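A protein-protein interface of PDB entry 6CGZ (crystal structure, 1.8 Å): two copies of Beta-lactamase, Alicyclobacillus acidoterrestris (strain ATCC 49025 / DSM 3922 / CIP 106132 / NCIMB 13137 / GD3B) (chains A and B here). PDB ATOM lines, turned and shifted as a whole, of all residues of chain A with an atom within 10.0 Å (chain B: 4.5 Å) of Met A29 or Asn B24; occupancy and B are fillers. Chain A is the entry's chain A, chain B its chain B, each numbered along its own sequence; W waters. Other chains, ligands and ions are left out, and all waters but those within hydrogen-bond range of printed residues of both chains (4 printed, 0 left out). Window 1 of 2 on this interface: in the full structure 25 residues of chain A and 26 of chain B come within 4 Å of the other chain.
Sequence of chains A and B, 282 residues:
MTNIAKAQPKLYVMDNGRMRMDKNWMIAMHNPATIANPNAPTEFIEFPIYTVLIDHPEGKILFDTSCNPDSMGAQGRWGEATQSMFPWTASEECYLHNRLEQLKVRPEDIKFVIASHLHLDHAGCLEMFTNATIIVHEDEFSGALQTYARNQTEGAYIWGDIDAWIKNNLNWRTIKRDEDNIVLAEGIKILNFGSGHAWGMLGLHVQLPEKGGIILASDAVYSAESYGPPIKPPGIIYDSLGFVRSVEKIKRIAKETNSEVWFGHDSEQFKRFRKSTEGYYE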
ATOM      1  N   ASP A  22      10.728  -1.701  12.578  1.00  0.00           N
ATOM      2  CA  ASP A  22      10.114  -0.394  12.410  1.00  0.00           C
ATOM      3  C   ASP A  22      11.191   0.656  12.493  1.00  0.00           C
ATOM      4  O   ASP A  22      11.965   0.670  13.447  1.00  0.00           O
ATOM      5  CB  ASP A  22       9.080  -0.233  13.526  1.00  0.00           C
ATOM      6  CG  ASP A  22       8.171   1.004  13.342  1.00  0.00           C
ATOM      7  OD1 ASP A  22       8.672   2.068  12.893  1.00  0.00           O
ATOM      8  OD2 ASP A  22       6.973   0.864  13.698  1.00  0.00           O
ATOM      9  N   LYS A  23      11.256   1.551  11.524  1.00  0.00           N
ATOM     10  CA  LYS A  23      12.275   2.581  11.562  1.00  0.00           C
ATOM     11  C   LYS A  23      12.180   3.432  12.835  1.00  0.00           C
ATOM     12  O   LYS A  23      13.190   3.954  13.295  1.00  0.00           O
ATOM     13  CB  LYS A  23      12.244   3.478  10.325  1.00  0.00           C
ATOM     14  CG  LYS A  23      13.391   4.463  10.353  1.00  0.00           C
ATOM     15  CD  LYS A  23      13.619   5.208   9.058  1.00  0.00           C
ATOM     16  CE  LYS A  23      14.730   6.204   9.271  1.00  0.00           C
ATOM     17  NZ  LYS A  23      15.428   6.595   8.026  1.00  0.00           N
ATOM     18  N   ASN A  24      11.001   3.549  13.427  1.00  0.00           N
ATOM     19  CA  ASN A  24      10.885   4.331  14.680  1.00  0.00           C
ATOM     20  C   ASN A  24      11.709   3.746  15.838  1.00  0.00           C
ATOM     21  O   ASN A  24      12.105   4.475  16.753  1.00  0.00           O
ATOM     22  CB  ASN A  24       9.426   4.496  15.112  1.00  0.00           C
ATOM     23  CG  ASN A  24       8.664   5.473  14.240  1.00  0.00           C
ATOM     24  OD1 ASN A  24       7.556   5.193  13.784  1.00  0.00           O
ATOM     25  ND2 ASN A  24       9.260   6.602  13.991  1.00  0.00           N
ATOM     26  N   TRP A  25      11.995   2.450  15.812  1.00  0.00           N
ATOM     27  CA  TRP A  25      12.879   1.883  16.845  1.00  0.00           C
ATOM     28  C   TRP A  25      14.265   2.484  16.684  1.00  0.00           C
ATOM     29  O   TRP A  25      14.958   2.721  17.667  1.00  0.00           O
ATOM     30  CB  TRP A  25      13.012   0.356  16.749  1.00  0.00           C
ATOM     31  CG  TRP A  25      11.808  -0.471  17.039  1.00  0.00           C
ATOM     32  CD1 TRP A  25      11.091  -1.227  16.140  1.00  0.00           C
ATOM     33  CD2 TRP A  25      11.214  -0.723  18.321  1.00  0.00           C
ATOM     34  NE1 TRP A  25      10.082  -1.899  16.775  1.00  0.00           N
ATOM     35  CE2 TRP A  25      10.126  -1.605  18.115  1.00  0.00           C
ATOM     36  CE3 TRP A  25      11.480  -0.271  19.625  1.00  0.00           C
ATOM     37  CZ2 TRP A  25       9.311  -2.049  19.162  1.00  0.00           C
ATOM     38  CZ3 TRP A  25      10.659  -0.727  20.666  1.00  0.00           C
ATOM     39  CH2 TRP A  25       9.593  -1.583  20.425  1.00  0.00           C
ATOM     40  N   MET A  26      14.693   2.723  15.440  1.00  0.00           N
ATOM     41  CA  MET A  26      16.017   3.235  15.206  1.00  0.00           C
ATOM     42  C   MET A  26      16.115   4.742  15.369  1.00  0.00           C
ATOM     43  O   MET A  26      17.033   5.236  16.008  1.00  0.00           O
ATOM     44  CB  MET A  26      16.540   2.845  13.822  1.00  0.00           C
ATOM     45  CG  MET A  26      18.009   3.168  13.658  1.00  0.00           C
ATOM     46  SD  MET A  26      18.794   2.654  12.106  1.00  0.00           S
ATOM     47  CE  MET A  26      18.874   0.874  12.401  1.00  0.00           C
ATOM     48  N   ILE A  27      15.166   5.469  14.798  1.00  0.00           N
ATOM     49  CA  ILE A  27      15.138   6.921  14.889  1.00  0.00           C
ATOM     50  C   ILE A  27      13.760   7.350  15.411  1.00  0.00           C
ATOM     51  O   ILE A  27      12.788   7.307  14.676  1.00  0.00           O
ATOM     52  CB  ILE A  27      15.364   7.541  13.502  1.00  0.00           C
ATOM     53  CG1 ILE A  27      16.697   7.080  12.887  1.00  0.00           C
ATOM     54  CG2 ILE A  27      15.221   9.048  13.551  1.00  0.00           C
ATOM     55  CD1 ILE A  27      17.945   7.506  13.614  1.00  0.00           C
ATOM     56  N   ALA A  28      13.684   7.744  16.687  1.00  0.00           N
ATOM     57  CA  ALA A  28      12.428   8.163  17.321  1.00  0.00           C
ATOM     58  C   ALA A  28      11.725   9.223  16.496  1.00  0.00           C
ATOM     59  O   ALA A  28      12.342  10.179  16.041  1.00  0.00           O
ATOM     60  CB  ALA A  28      12.658   8.689  18.714  1.00  0.00           C
ATOM     61  N   MET A  29      10.429   9.021  16.305  1.00  0.00           N
ATOM     62  CA  MET A  29       9.577   9.981  15.629  1.00  0.00           C
ATOM     63  C   MET A  29      10.175  10.476  14.324  1.00  0.00           C
ATOM     64  O   MET A  29      10.146  11.649  14.019  1.00  0.00           O
ATOM     65  CB  MET A  29       9.284  11.168  16.584  1.00  0.00           C
ATOM     66  CG  MET A  29       8.662  10.760  17.903  1.00  0.00           C
ATOM     67  SD  MET A  29       7.140   9.810  17.782  1.00  0.00           S
ATOM     68  CE  MET A  29       6.167  10.840  16.667  1.00  0.00           C
ATOM     69  N   HIS A  30      10.676   9.559  13.512  1.00  0.00           N
ATOM     70  CA  HIS A  30      11.331   9.944  12.282  1.00  0.00           C
ATOM     71  C   HIS A  30      10.369  10.540  11.267  1.00  0.00           C
ATOM     72  O   HIS A  30      10.808  11.251  10.366  1.00  0.00           O
ATOM     73  CB  HIS A  30      12.043   8.728  11.633  1.00  0.00           C
ATOM     74  CG  HIS A  30      11.127   7.820  10.882  1.00  0.00           C
ATOM     75  ND1 HIS A  30      11.064   7.803   9.504  1.00  0.00           N
ATOM     76  CD2 HIS A  30      10.242   6.892  11.310  1.00  0.00           C
ATOM     77  CE1 HIS A  30      10.164   6.920   9.119  1.00  0.00           C
ATOM     78  NE2 HIS A  30       9.653   6.350  10.195  1.00  0.00           N
ATOM     79  N   ASN A  31       9.078  10.221  11.366  1.00  0.00           N
ATOM     80  CA  ASN A  31       8.101  10.746  10.397  1.00  0.00           C
ATOM     81  C   ASN A  31       6.732  10.988  11.034  1.00  0.00           C
ATOM     82  O   ASN A  31       5.794  10.253  10.785  1.00  0.00           O
ATOM     83  CB  ASN A  31       7.946   9.770   9.232  1.00  0.00           C
ATOM     84  CG  ASN A  31       7.064  10.313   8.137  1.00  0.00           C
ATOM     85  OD1 ASN A  31       7.129  11.495   7.809  1.00  0.00           O
ATOM     86  ND2 ASN A  31       6.226   9.458   7.577  1.00  0.00           N
ATOM     87  N   PRO A  32       6.637  12.026  11.880  1.00  0.00           N
ATOM     88  CA  PRO A  32       5.429  12.191  12.654  1.00  0.00           C
ATOM     89  C   PRO A  32       4.193  12.531  11.820  1.00  0.00           C
ATOM     90  O   PRO A  32       4.293  13.225  10.824  1.00  0.00           O
ATOM     91  CB  PRO A  32       5.773  13.343  13.622  1.00  0.00           C
ATOM     92  CG  PRO A  32       7.251  13.503  13.559  1.00  0.00           C
ATOM     93  CD  PRO A  32       7.636  13.064  12.173  1.00  0.00           C
ATOM     94  N   ALA A  33       3.055  12.020  12.248  1.00  0.00           N
ATOM     95  CA  ALA A  33       1.765  12.374  11.670  1.00  0.00           C
ATOM     96  C   ALA A  33       1.557  13.882  11.771  1.00  0.00           C
ATOM     97  O   ALA A  33       2.012  14.546  12.722  1.00  0.00           O
ATOM     98  CB  ALA A  33       0.653  11.638  12.384  1.00  0.00           C
ATOM     99  N   THR A  34       0.902  14.429  10.751  1.00  0.00           N
ATOM    100  CA  THR A  34       0.631  15.847  10.671  1.00  0.00           C
ATOM    101  C   THR A  34      -0.794  16.005  10.169  1.00  0.00           C
ATOM    102  O   THR A  34      -1.499  15.009   9.889  1.00  0.00           O
ATOM    103  CB  THR A  34       1.560  16.580   9.682  1.00  0.00           C
ATOM    104  OG1 THR A  34       1.336  16.063   8.370  1.00  0.00           O
ATOM    105  CG2 THR A  34       3.009  16.424  10.031  1.00  0.00           C
ATOM    106  N   PRO A  38      -2.296  12.470   8.594  1.00  0.00           N
ATOM    107  CA  PRO A  38      -2.683  12.023   9.932  1.00  0.00           C
ATOM    108  C   PRO A  38      -2.334  10.580  10.233  1.00  0.00           C
ATOM    109  O   PRO A  38      -2.284  10.200  11.404  1.00  0.00           O
ATOM    110  CB  PRO A  38      -4.207  12.180   9.945  1.00  0.00           C
ATOM    111  CG  PRO A  38      -4.619  12.271   8.502  1.00  0.00           C
ATOM    112  CD  PRO A  38      -3.466  12.841   7.760  1.00  0.00           C
ATOM    113  N   ASN A  39      -2.127   9.774   9.196  1.00  0.00           N
ATOM    114  CA  ASN A  39      -1.824   8.359   9.402  1.00  0.00           C
ATOM    115  C   ASN A  39      -0.455   8.026   8.809  1.00  0.00           C
ATOM    116  O   ASN A  39      -0.270   7.010   8.140  1.00  0.00           O
ATOM    117  CB  ASN A  39      -2.906   7.483   8.792  1.00  0.00           C
ATOM    118  CG  ASN A  39      -4.279   7.810   9.323  1.00  0.00           C
ATOM    119  OD1 ASN A  39      -4.586   7.603  10.506  1.00  0.00           O
ATOM    120  ND2 ASN A  39      -5.117   8.334   8.452  1.00  0.00           N
ATOM    121  N   ALA A  40       0.498   8.906   9.059  1.00  0.00           N
ATOM    122  CA  ALA A  40       1.822   8.801   8.494  1.00  0.00           C
ATOM    123  C   ALA A  40       2.314   7.350   8.620  1.00  0.00           C
ATOM    124  O   ALA A  40       2.337   6.785   9.706  1.00  0.00           O
ATOM    125  CB  ALA A  40       2.766   9.775   9.190  1.00  0.00           C
ATOM    126  N   PRO A  41       2.650   6.732   7.486  1.00  0.00           N
ATOM    127  CA  PRO A  41       3.083   5.337   7.547  1.00  0.00           C
ATOM    128  C   PRO A  41       4.528   5.278   8.014  1.00  0.00           C
ATOM    129  O   PRO A  41       5.310   6.193   7.742  1.00  0.00           O
ATOM    130  CB  PRO A  41       2.989   4.894   6.083  1.00  0.00           C
ATOM    131  CG  PRO A  41       3.325   6.141   5.305  1.00  0.00           C
ATOM    132  CD  PRO A  41       2.902   7.328   6.154  1.00  0.00           C
ATOM    133  N   THR A  42       4.898   4.221   8.719  1.00  0.00           N
ATOM    134  CA  THR A  42       6.305   4.051   9.018  1.00  0.00           C
ATOM    135  C   THR A  42       6.906   3.155   7.934  1.00  0.00           C
ATOM    136  O   THR A  42       6.235   2.835   6.939  1.00  0.00           O
ATOM    137  CB  THR A  42       6.541   3.457  10.426  1.00  0.00           C
ATOM    138  OG1 THR A  42       7.949   3.454  10.708  1.00  0.00           O
ATOM    139  CG2 THR A  42       5.970   2.059  10.527  1.00  0.00           C
ATOM    140  N   GLU A  43       8.164   2.779   8.101  1.00  0.00           N
ATOM    141  CA  GLU A  43       8.771   1.813   7.188  1.00  0.00           C
ATOM    142  C   GLU A  43       9.532   0.732   7.988  1.00  0.00           C
ATOM    143  O   GLU A  43       9.932   0.955   9.136  1.00  0.00           O
ATOM    144  CB  GLU A  43       9.639   2.520   6.137  1.00  0.00           C
ATOM    145  CG  GLU A  43      11.027   2.959   6.589  1.00  0.00           C
ATOM    146  CD  GLU A  43      11.708   3.917   5.600  1.00  0.00           C
ATOM    147  OE1 GLU A  43      12.478   3.442   4.730  1.00  0.00           O
ATOM    148  OE2 GLU A  43      11.465   5.143   5.694  1.00  0.00           O
ATOM    149  N   GLU A 225      22.730   8.444  10.877  1.00  0.00           N
ATOM    150  CA  GLU A 225      21.588   9.280  11.161  1.00  0.00           C
ATOM    151  C   GLU A 225      21.447   9.538  12.664  1.00  0.00           C
ATOM    152  O   GLU A 225      21.141  10.656  13.067  1.00  0.00           O
ATOM    153  CB  GLU A 225      20.318   8.654  10.616  1.00  0.00           C
ATOM    154  CG  GLU A 225      19.157   9.620  10.547  1.00  0.00           C
ATOM    155  CD  GLU A 225      17.933   9.032   9.860  1.00  0.00           C
ATOM    156  OE1 GLU A 225      18.004   7.889   9.343  1.00  0.00           O
ATOM    157  OE2 GLU A 225      16.880   9.709   9.885  1.00  0.00           O
ATOM    158  N   LYS A 232      20.125  11.918  17.066  1.00  0.00           N
ATOM    159  CA  LYS A 232      18.734  11.467  17.025  1.00  0.00           C
ATOM    160  C   LYS A 232      18.601  10.176  17.806  1.00  0.00           C
ATOM    161  O   LYS A 232      19.139   9.144  17.389  1.00  0.00           O
ATOM    162  CB  LYS A 232      18.261  11.262  15.587  1.00  0.00           C
ATOM    163  CG  LYS A 232      18.159  12.552  14.770  1.00  0.00           C
ATOM    164  CD  LYS A 232      17.714  12.305  13.336  1.00  0.00           C
ATOM    165  CE  LYS A 232      17.436  13.609  12.591  1.00  0.00           C
ATOM    166  NZ  LYS A 232      17.057  13.295  11.182  1.00  0.00           N
ATOM    167  N   PRO A 233      17.881  10.209  18.931  1.00  0.00           N
ATOM    168  CA  PRO A 233      17.825   9.011  19.755  1.00  0.00           C
ATOM    169  C   PRO A 233      16.853   7.970  19.199  1.00  0.00           C
ATOM    170  O   PRO A 233      16.006   8.287  18.348  1.00  0.00           O
ATOM    171  CB  PRO A 233      17.320   9.548  21.112  1.00  0.00           C
ATOM    172  CG  PRO A 233      16.403  10.657  20.700  1.00  0.00           C
ATOM    173  CD  PRO A 233      17.069  11.301  19.506  1.00  0.00           C
ATOM    174  N   PRO A 234      16.977   6.732  19.668  1.00  0.00           N
ATOM    175  CA  PRO A 234      16.089   5.632  19.290  1.00  0.00           C
ATOM    176  C   PRO A 234      14.701   5.776  19.898  1.00  0.00           C
ATOM    177  O   PRO A 234      14.534   6.530  20.853  1.00  0.00           O
ATOM    178  CB  PRO A 234      16.780   4.381  19.855  1.00  0.00           C
ATOM    179  CG  PRO A 234      17.952   4.843  20.625  1.00  0.00           C
ATOM    180  CD  PRO A 234      18.046   6.322  20.594  1.00  0.00           C
ATOM    181  N   GLY A 235      13.739   5.028  19.360  1.00  0.00           N
ATOM    182  CA  GLY A 235      12.301   5.202  19.660  1.00  0.00           C
ATOM    183  C   GLY A 235      11.916   4.899  21.094  1.00  0.00           C
ATOM    184  O   GLY A 235      11.039   5.560  21.689  1.00  0.00           O
ATOM    185  N   ILE A 236      12.529   3.864  21.631  1.00  0.00           N
ATOM    186  CA  ILE A 236      12.412   3.623  23.047  1.00  0.00           C
ATOM    187  C   ILE A 236      13.844   3.546  23.526  1.00  0.00           C
ATOM    188  O   ILE A 236      14.679   2.857  22.929  1.00  0.00           O
ATOM    189  CB  ILE A 236      11.577   2.382  23.372  1.00  0.00           C
ATOM    190  CG1 ILE A 236      10.117   2.825  23.525  1.00  0.00           C
ATOM    191  CG2 ILE A 236      12.048   1.739  24.668  1.00  0.00           C
ATOM    192  CD1 ILE A 236       9.118   1.689  23.556  1.00  0.00           C
ATOM    193  N   ASP B  22       0.332  12.843  16.663  1.00  0.00           N
ATOM    194  CA  ASP B  22       0.703  11.445  16.445  1.00  0.00           C
ATOM    195  C   ASP B  22       0.623  10.705  17.784  1.00  0.00           C
ATOM    196  O   ASP B  22       1.197  11.142  18.781  1.00  0.00           O
ATOM    197  CB  ASP B  22       2.111  11.407  15.867  1.00  0.00           C
ATOM    198  CG  ASP B  22       2.491  10.030  15.287  1.00  0.00           C
ATOM    199  OD1 ASP B  22       2.087   8.996  15.858  1.00  0.00           O
ATOM    200  OD2 ASP B  22       3.231  10.033  14.295  1.00  0.00           O
ATOM    201  N   LYS B  23      -0.102   9.603  17.803  1.00  0.00           N
ATOM    202  CA  LYS B  23      -0.225   8.841  19.022  1.00  0.00           C
ATOM    203  C   LYS B  23       1.140   8.384  19.527  1.00  0.00           C
ATOM    204  O   LYS B  23       1.326   8.202  20.736  1.00  0.00           O
ATOM    205  CB  LYS B  23      -1.153   7.654  18.849  1.00  0.00           C
ATOM    206  CG  LYS B  23      -1.243   6.878  20.145  1.00  0.00           C
ATOM    207  CD  LYS B  23      -2.446   5.998  20.281  1.00  0.00           C
ATOM    208  CE  LYS B  23      -2.342   5.277  21.599  1.00  0.00           C
ATOM    209  NZ  LYS B  23      -3.665   5.006  22.195  1.00  0.00           N
ATOM    210  N   ASN B  24       2.099   8.218  18.623  1.00  0.00           N
ATOM    211  CA  ASN B  24       3.449   7.846  19.057  1.00  0.00           C
ATOM    212  C   ASN B  24       4.094   8.858  20.002  1.00  0.00           C
ATOM    213  O   ASN B  24       4.963   8.485  20.798  1.00  0.00           O
ATOM    214  CB  ASN B  24       4.368   7.573  17.881  1.00  0.00           C
ATOM    215  CG  ASN B  24       4.118   6.212  17.253  1.00  0.00           C
ATOM    216  OD1 ASN B  24       4.057   6.081  16.024  1.00  0.00           O
ATOM    217  ND2 ASN B  24       3.984   5.198  18.082  1.00  0.00           N
ATOM    218  N   TRP B  25       3.686  10.119  19.933  1.00  0.00           N
ATOM    219  CA  TRP B  25       4.209  11.103  20.859  1.00  0.00           C
ATOM    220  C   TRP B  25       3.721  10.804  22.247  1.00  0.00           C
ATOM    221  O   TRP B  25       4.442  11.079  23.215  1.00  0.00           O
ATOM    222  CB  TRP B  25       3.755  12.524  20.542  1.00  0.00           C
ATOM    223  CG  TRP B  25       4.234  13.144  19.272  1.00  0.00           C
ATOM    224  CD1 TRP B  25       3.475  13.430  18.168  1.00  0.00           C
ATOM    225  CD2 TRP B  25       5.544  13.659  18.993  1.00  0.00           C
ATOM    226  NE1 TRP B  25       4.237  14.047  17.212  1.00  0.00           N
ATOM    227  CE2 TRP B  25       5.505  14.217  17.688  1.00  0.00           C
ATOM    228  CE3 TRP B  25       6.746  13.697  19.705  1.00  0.00           C
ATOM    229  CZ2 TRP B  25       6.618  14.791  17.085  1.00  0.00           C
ATOM    230  CZ3 TRP B  25       7.852  14.277  19.104  1.00  0.00           C
ATOM    231  CH2 TRP B  25       7.780  14.812  17.802  1.00  0.00           C
ATOM    232  N   MET B  26       2.475  10.339  22.360  1.00  0.00           N
ATOM    233  CA  MET B  26       1.872  10.068  23.661  1.00  0.00           C
ATOM    234  C   MET B  26       2.310   8.730  24.225  1.00  0.00           C
ATOM    235  O   MET B  26       2.698   8.641  25.391  1.00  0.00           O
ATOM    236  CB  MET B  26       0.351  10.139  23.615  1.00  0.00           C
ATOM    237  CG  MET B  26      -0.239  10.059  25.022  1.00  0.00           C
ATOM    238  SD  MET B  26      -2.007  10.333  25.131  1.00  0.00           S
ATOM    239  CE  MET B  26      -1.977  12.089  24.726  1.00  0.00           C
ATOM    240  N   ILE B  27       2.306   7.709  23.374  1.00  0.00           N
ATOM    241  CA  ILE B  27       2.691   6.352  23.783  1.00  0.00           C
ATOM    242  C   ILE B  27       3.728   5.823  22.800  1.00  0.00           C
ATOM    243  O   ILE B  27       3.388   5.443  21.680  1.00  0.00           O
ATOM    244  CB  ILE B  27       1.493   5.402  23.797  1.00  0.00           C
ATOM    245  CG1 ILE B  27       0.396   5.941  24.722  1.00  0.00           C
ATOM    246  CG2 ILE B  27       1.916   3.985  24.176  1.00  0.00           C
ATOM    247  CD1 ILE B  27       0.721   5.891  26.200  1.00  0.00           C
ATOM    248  N   ALA B  28       4.988   5.858  23.217  1.00  0.00           N
ATOM    249  CA  ALA B  28       6.108   5.463  22.352  1.00  0.00           C
ATOM    250  C   ALA B  28       5.855   4.081  21.784  1.00  0.00           C
ATOM    251  O   ALA B  28       5.431   3.179  22.495  1.00  0.00           O
ATOM    252  CB  ALA B  28       7.422   5.480  23.119  1.00  0.00           C
ATOM    253  N   MET B  29       6.104   3.944  20.480  1.00  0.00           N
ATOM    254  CA  MET B  29       5.996   2.674  19.778  1.00  0.00           C
ATOM    255  C   MET B  29       4.708   1.944  20.081  1.00  0.00           C
ATOM    256  O   MET B  29       4.721   0.747  20.344  1.00  0.00           O
ATOM    257  CB  MET B  29       7.189   1.779  20.156  1.00  0.00           C
ATOM    258  CG  MET B  29       8.555   2.398  19.857  1.00  0.00           C
ATOM    259  SD  MET B  29       8.810   2.967  18.154  1.00  0.00           S
ATOM    260  CE  MET B  29       8.256   1.508  17.275  1.00  0.00           C
ATOM    261  N   HIS B  30       3.583   2.655  20.033  1.00  0.00           N
ATOM    262  CA  HIS B  30       2.302   2.054  20.372  1.00  0.00           C
ATOM    263  C   HIS B  30       1.822   0.980  19.404  1.00  0.00           C
ATOM    264  O   HIS B  30       1.020   0.150  19.796  1.00  0.00           O
ATOM    265  CB  HIS B  30       1.202   3.124  20.513  1.00  0.00           C
ATOM    266  CG  HIS B  30       0.656   3.604  19.204  1.00  0.00           C
ATOM    267  ND1 HIS B  30      -0.579   3.221  18.728  1.00  0.00           N
ATOM    268  CD2 HIS B  30       1.172   4.434  18.274  1.00  0.00           C
ATOM    269  CE1 HIS B  30      -0.796   3.788  17.556  1.00  0.00           C
ATOM    270  NE2 HIS B  30       0.255   4.525  17.254  1.00  0.00           N
ATOM    271  N   THR B  42       0.140   5.152  11.743  1.00  0.00           N
ATOM    272  CA  THR B  42      -0.157   5.683  13.077  1.00  0.00           C
ATOM    273  C   THR B  42      -1.545   6.353  13.076  1.00  0.00           C
ATOM    274  O   THR B  42      -2.223   6.379  12.045  1.00  0.00           O
ATOM    275  CB  THR B  42       0.940   6.654  13.599  1.00  0.00           C
ATOM    276  OG1 THR B  42       0.698   6.948  15.000  1.00  0.00           O
ATOM    277  CG2 THR B  42       1.005   7.931  12.763  1.00  0.00           C
ATOM    278  N   PRO B 234       6.383   8.314  26.809  1.00  0.00           N
ATOM    279  CA  PRO B 234       6.065   9.047  25.597  1.00  0.00           C
ATOM    280  C   PRO B 234       7.149   8.886  24.536  1.00  0.00           C
ATOM    281  O   PRO B 234       8.247   8.434  24.851  1.00  0.00           O
ATOM    282  CB  PRO B 234       5.956  10.491  26.082  1.00  0.00           C
ATOM    283  CG  PRO B 234       6.742  10.546  27.324  1.00  0.00           C
ATOM    284  CD  PRO B 234       6.633   9.201  27.957  1.00  0.00           C
ATOM    285  N   GLY B 235       6.831   9.251  23.292  1.00  0.00           N
ATOM    286  CA  GLY B 235       7.685   8.936  22.131  1.00  0.00           C
ATOM    287  C   GLY B 235       8.976   9.711  22.026  1.00  0.00           C
ATOM    288  O   GLY B 235       9.947   9.237  21.416  1.00  0.00           O
ATOM    289  N   ILE B 236       8.989  10.929  22.545  1.00  0.00           N
ATOM    290  CA  ILE B 236      10.255  11.610  22.736  1.00  0.00           C
ATOM    291  C   ILE B 236      10.235  11.924  24.222  1.00  0.00           C
ATOM    292  O   ILE B 236       9.173  12.162  24.809  1.00  0.00           O
ATOM    293  CB  ILE B 236      10.437  12.881  21.863  1.00  0.00           C
ATOM    294  CG1 ILE B 236      10.670  12.527  20.394  1.00  0.00           C
ATOM    295  CG2 ILE B 236      11.656  13.679  22.329  1.00  0.00           C
ATOM    296  CD1 ILE B 236      12.060  12.004  20.094  1.00  0.00           C
HETATM  297  O   HOH W   1       2.183  14.862  15.429  1.00  0.00           O
HETATM  298  O   HOH W   2      12.902   8.404  22.654  1.00  0.00           O
HETATM  299  O   HOH W   3       7.335   6.250  19.028  1.00  0.00           O
HETATM  300  O   HOH W   4       9.642   6.909  20.256  1.00  0.00           O
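Asn B24 touches just one residue of chain A: Met A29. Asp B22 touches just these residues of chain A: Met A29, Pro A32 and Ala A33. Of chain A, only Gly A235 (3.9 Å) and Ile A236 (3.8 Å) come within 4 Å of Ala B28. Of chain A, only Asp A22 (3.9 Å), Asn A24 (3.5 Å), Trp A25 (3.7 Å) and Ile A236 (3.8 Å) come within 4 Å of Met B29. Of the printed residues of chain B, Trp A25 touches Met B29. Of the printed residues of chain A, Thr B42 touches Ala A33, Pro A38, Asn A39 and Ala A40. Printed residues of chain B within 4 Å of Asn A24: Met B29 (3.5 Å). Of the printed residues of chain B, Gly A235 touches Ala B28 (3.9 Å) and Gly B235 (3.8 Å). The nearest residue of chain B that does not touch Met A29 is Gly B235 (4.04 Å). The nearest residue of chain A that does not touch Asn B24 is Asn A24 (4.2 Å).
ND2 of Asn A24 lies close to N of His A30, at 3.3 Å. The backbone carbonyl oxygen of Asn A24 sits close to the backbone NH of Gly A235 (3.1 Å). The backbone NH (N) of Ala A28 lies within hydrogen-bond range of the backbone carbonyl oxygen (O) of Pro A233. The side-chain hydroxyl (OG1) of Thr B42 lies within hydrogen-bond range of the side-chain carboxylate (OD1) of Asp B22 (2.6 Å).
Of the 13 printed residues of chain B, 8 touch a printed residue of chain A. Hydrophobic or aromatic side chains of chain B within 4 Å of the printed part of chain A: Trp B25, Ala B28, Met B29 and Ile B236. Printed residues of chain A that touch a printed residue of chain B: Asp A22, Asn A24, Trp A25, Ala A28, Met A29, Pro A32, Ala A33, Pro A38, Asn A39, Ala A40, Gly A235 and Ile A236. Among the printed residues, no Asp or Glu carboxylate lies within 4 Å of a Lys or Arg side-chain nitrogen of the other chain.
Asp A22 touches Met B29, and with the chains exchanged Met A29 touches Asp B22. Trp A25 touches Met B29, and with the chains exchanged Met A29 touches Trp B25. Ala A28 touches Ile B236, and with the chains exchanged Ile A236 touches Ala B28. Gly B235 touches its own counterpart, Gly A235. Positions printed for both chains: 22, 23, 24, 25, 26, 27, 28, 29, 30, 42, 234, 235 and 236.
The backbone NH (N) of Ala A33 sits at hydrogen-bond distance from the side-chain carboxylate (OD2) of Asp B22, 2.9 Å away. OD1 of Asn A39 sits close to O of Thr B42, 3.1 Å away. The backbone carbonyl oxygen of Ala A40 is in hydrogen-bond range of the backbone NH of Thr B42 (3.4 Å).
Asp A22 touches Met B29. Asn A24 touches Met B29. Ala A28 touches Gly B235 (CB to O, 3.9 Å). Asp B22 touches Met A29. Ile B236 touches Met A29 (CG1 to CG, 3.7 Å). CB of Ala A33 touches CG2 of Thr B42 (3.7 Å). O of Thr B42 touches O of Pro A38, at 3.9 Å. O of Gly A235 touches CB of Ala B28 (3.9 Å). Ala B28 touches Ile A236 (CB to CG1, 3.8 Å). Ile A236 touches Met B29.
Water W4 bridges O of Gly A235 (2.4 Å) and O of Gly B235 (2.6 Å). Water W1 lies within hydrogen-bond range of O of Ala A33 (2.7 Å), NE1 of Trp B25 (2.8 Å) and N of Asp B22 (3.0 Å). Water W2 lies within hydrogen-bond range of the backbone carbonyl oxygen of Pro A234 (3.1 Å) and the backbone carbonyl oxygen of Gly B235 (3.3 Å).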
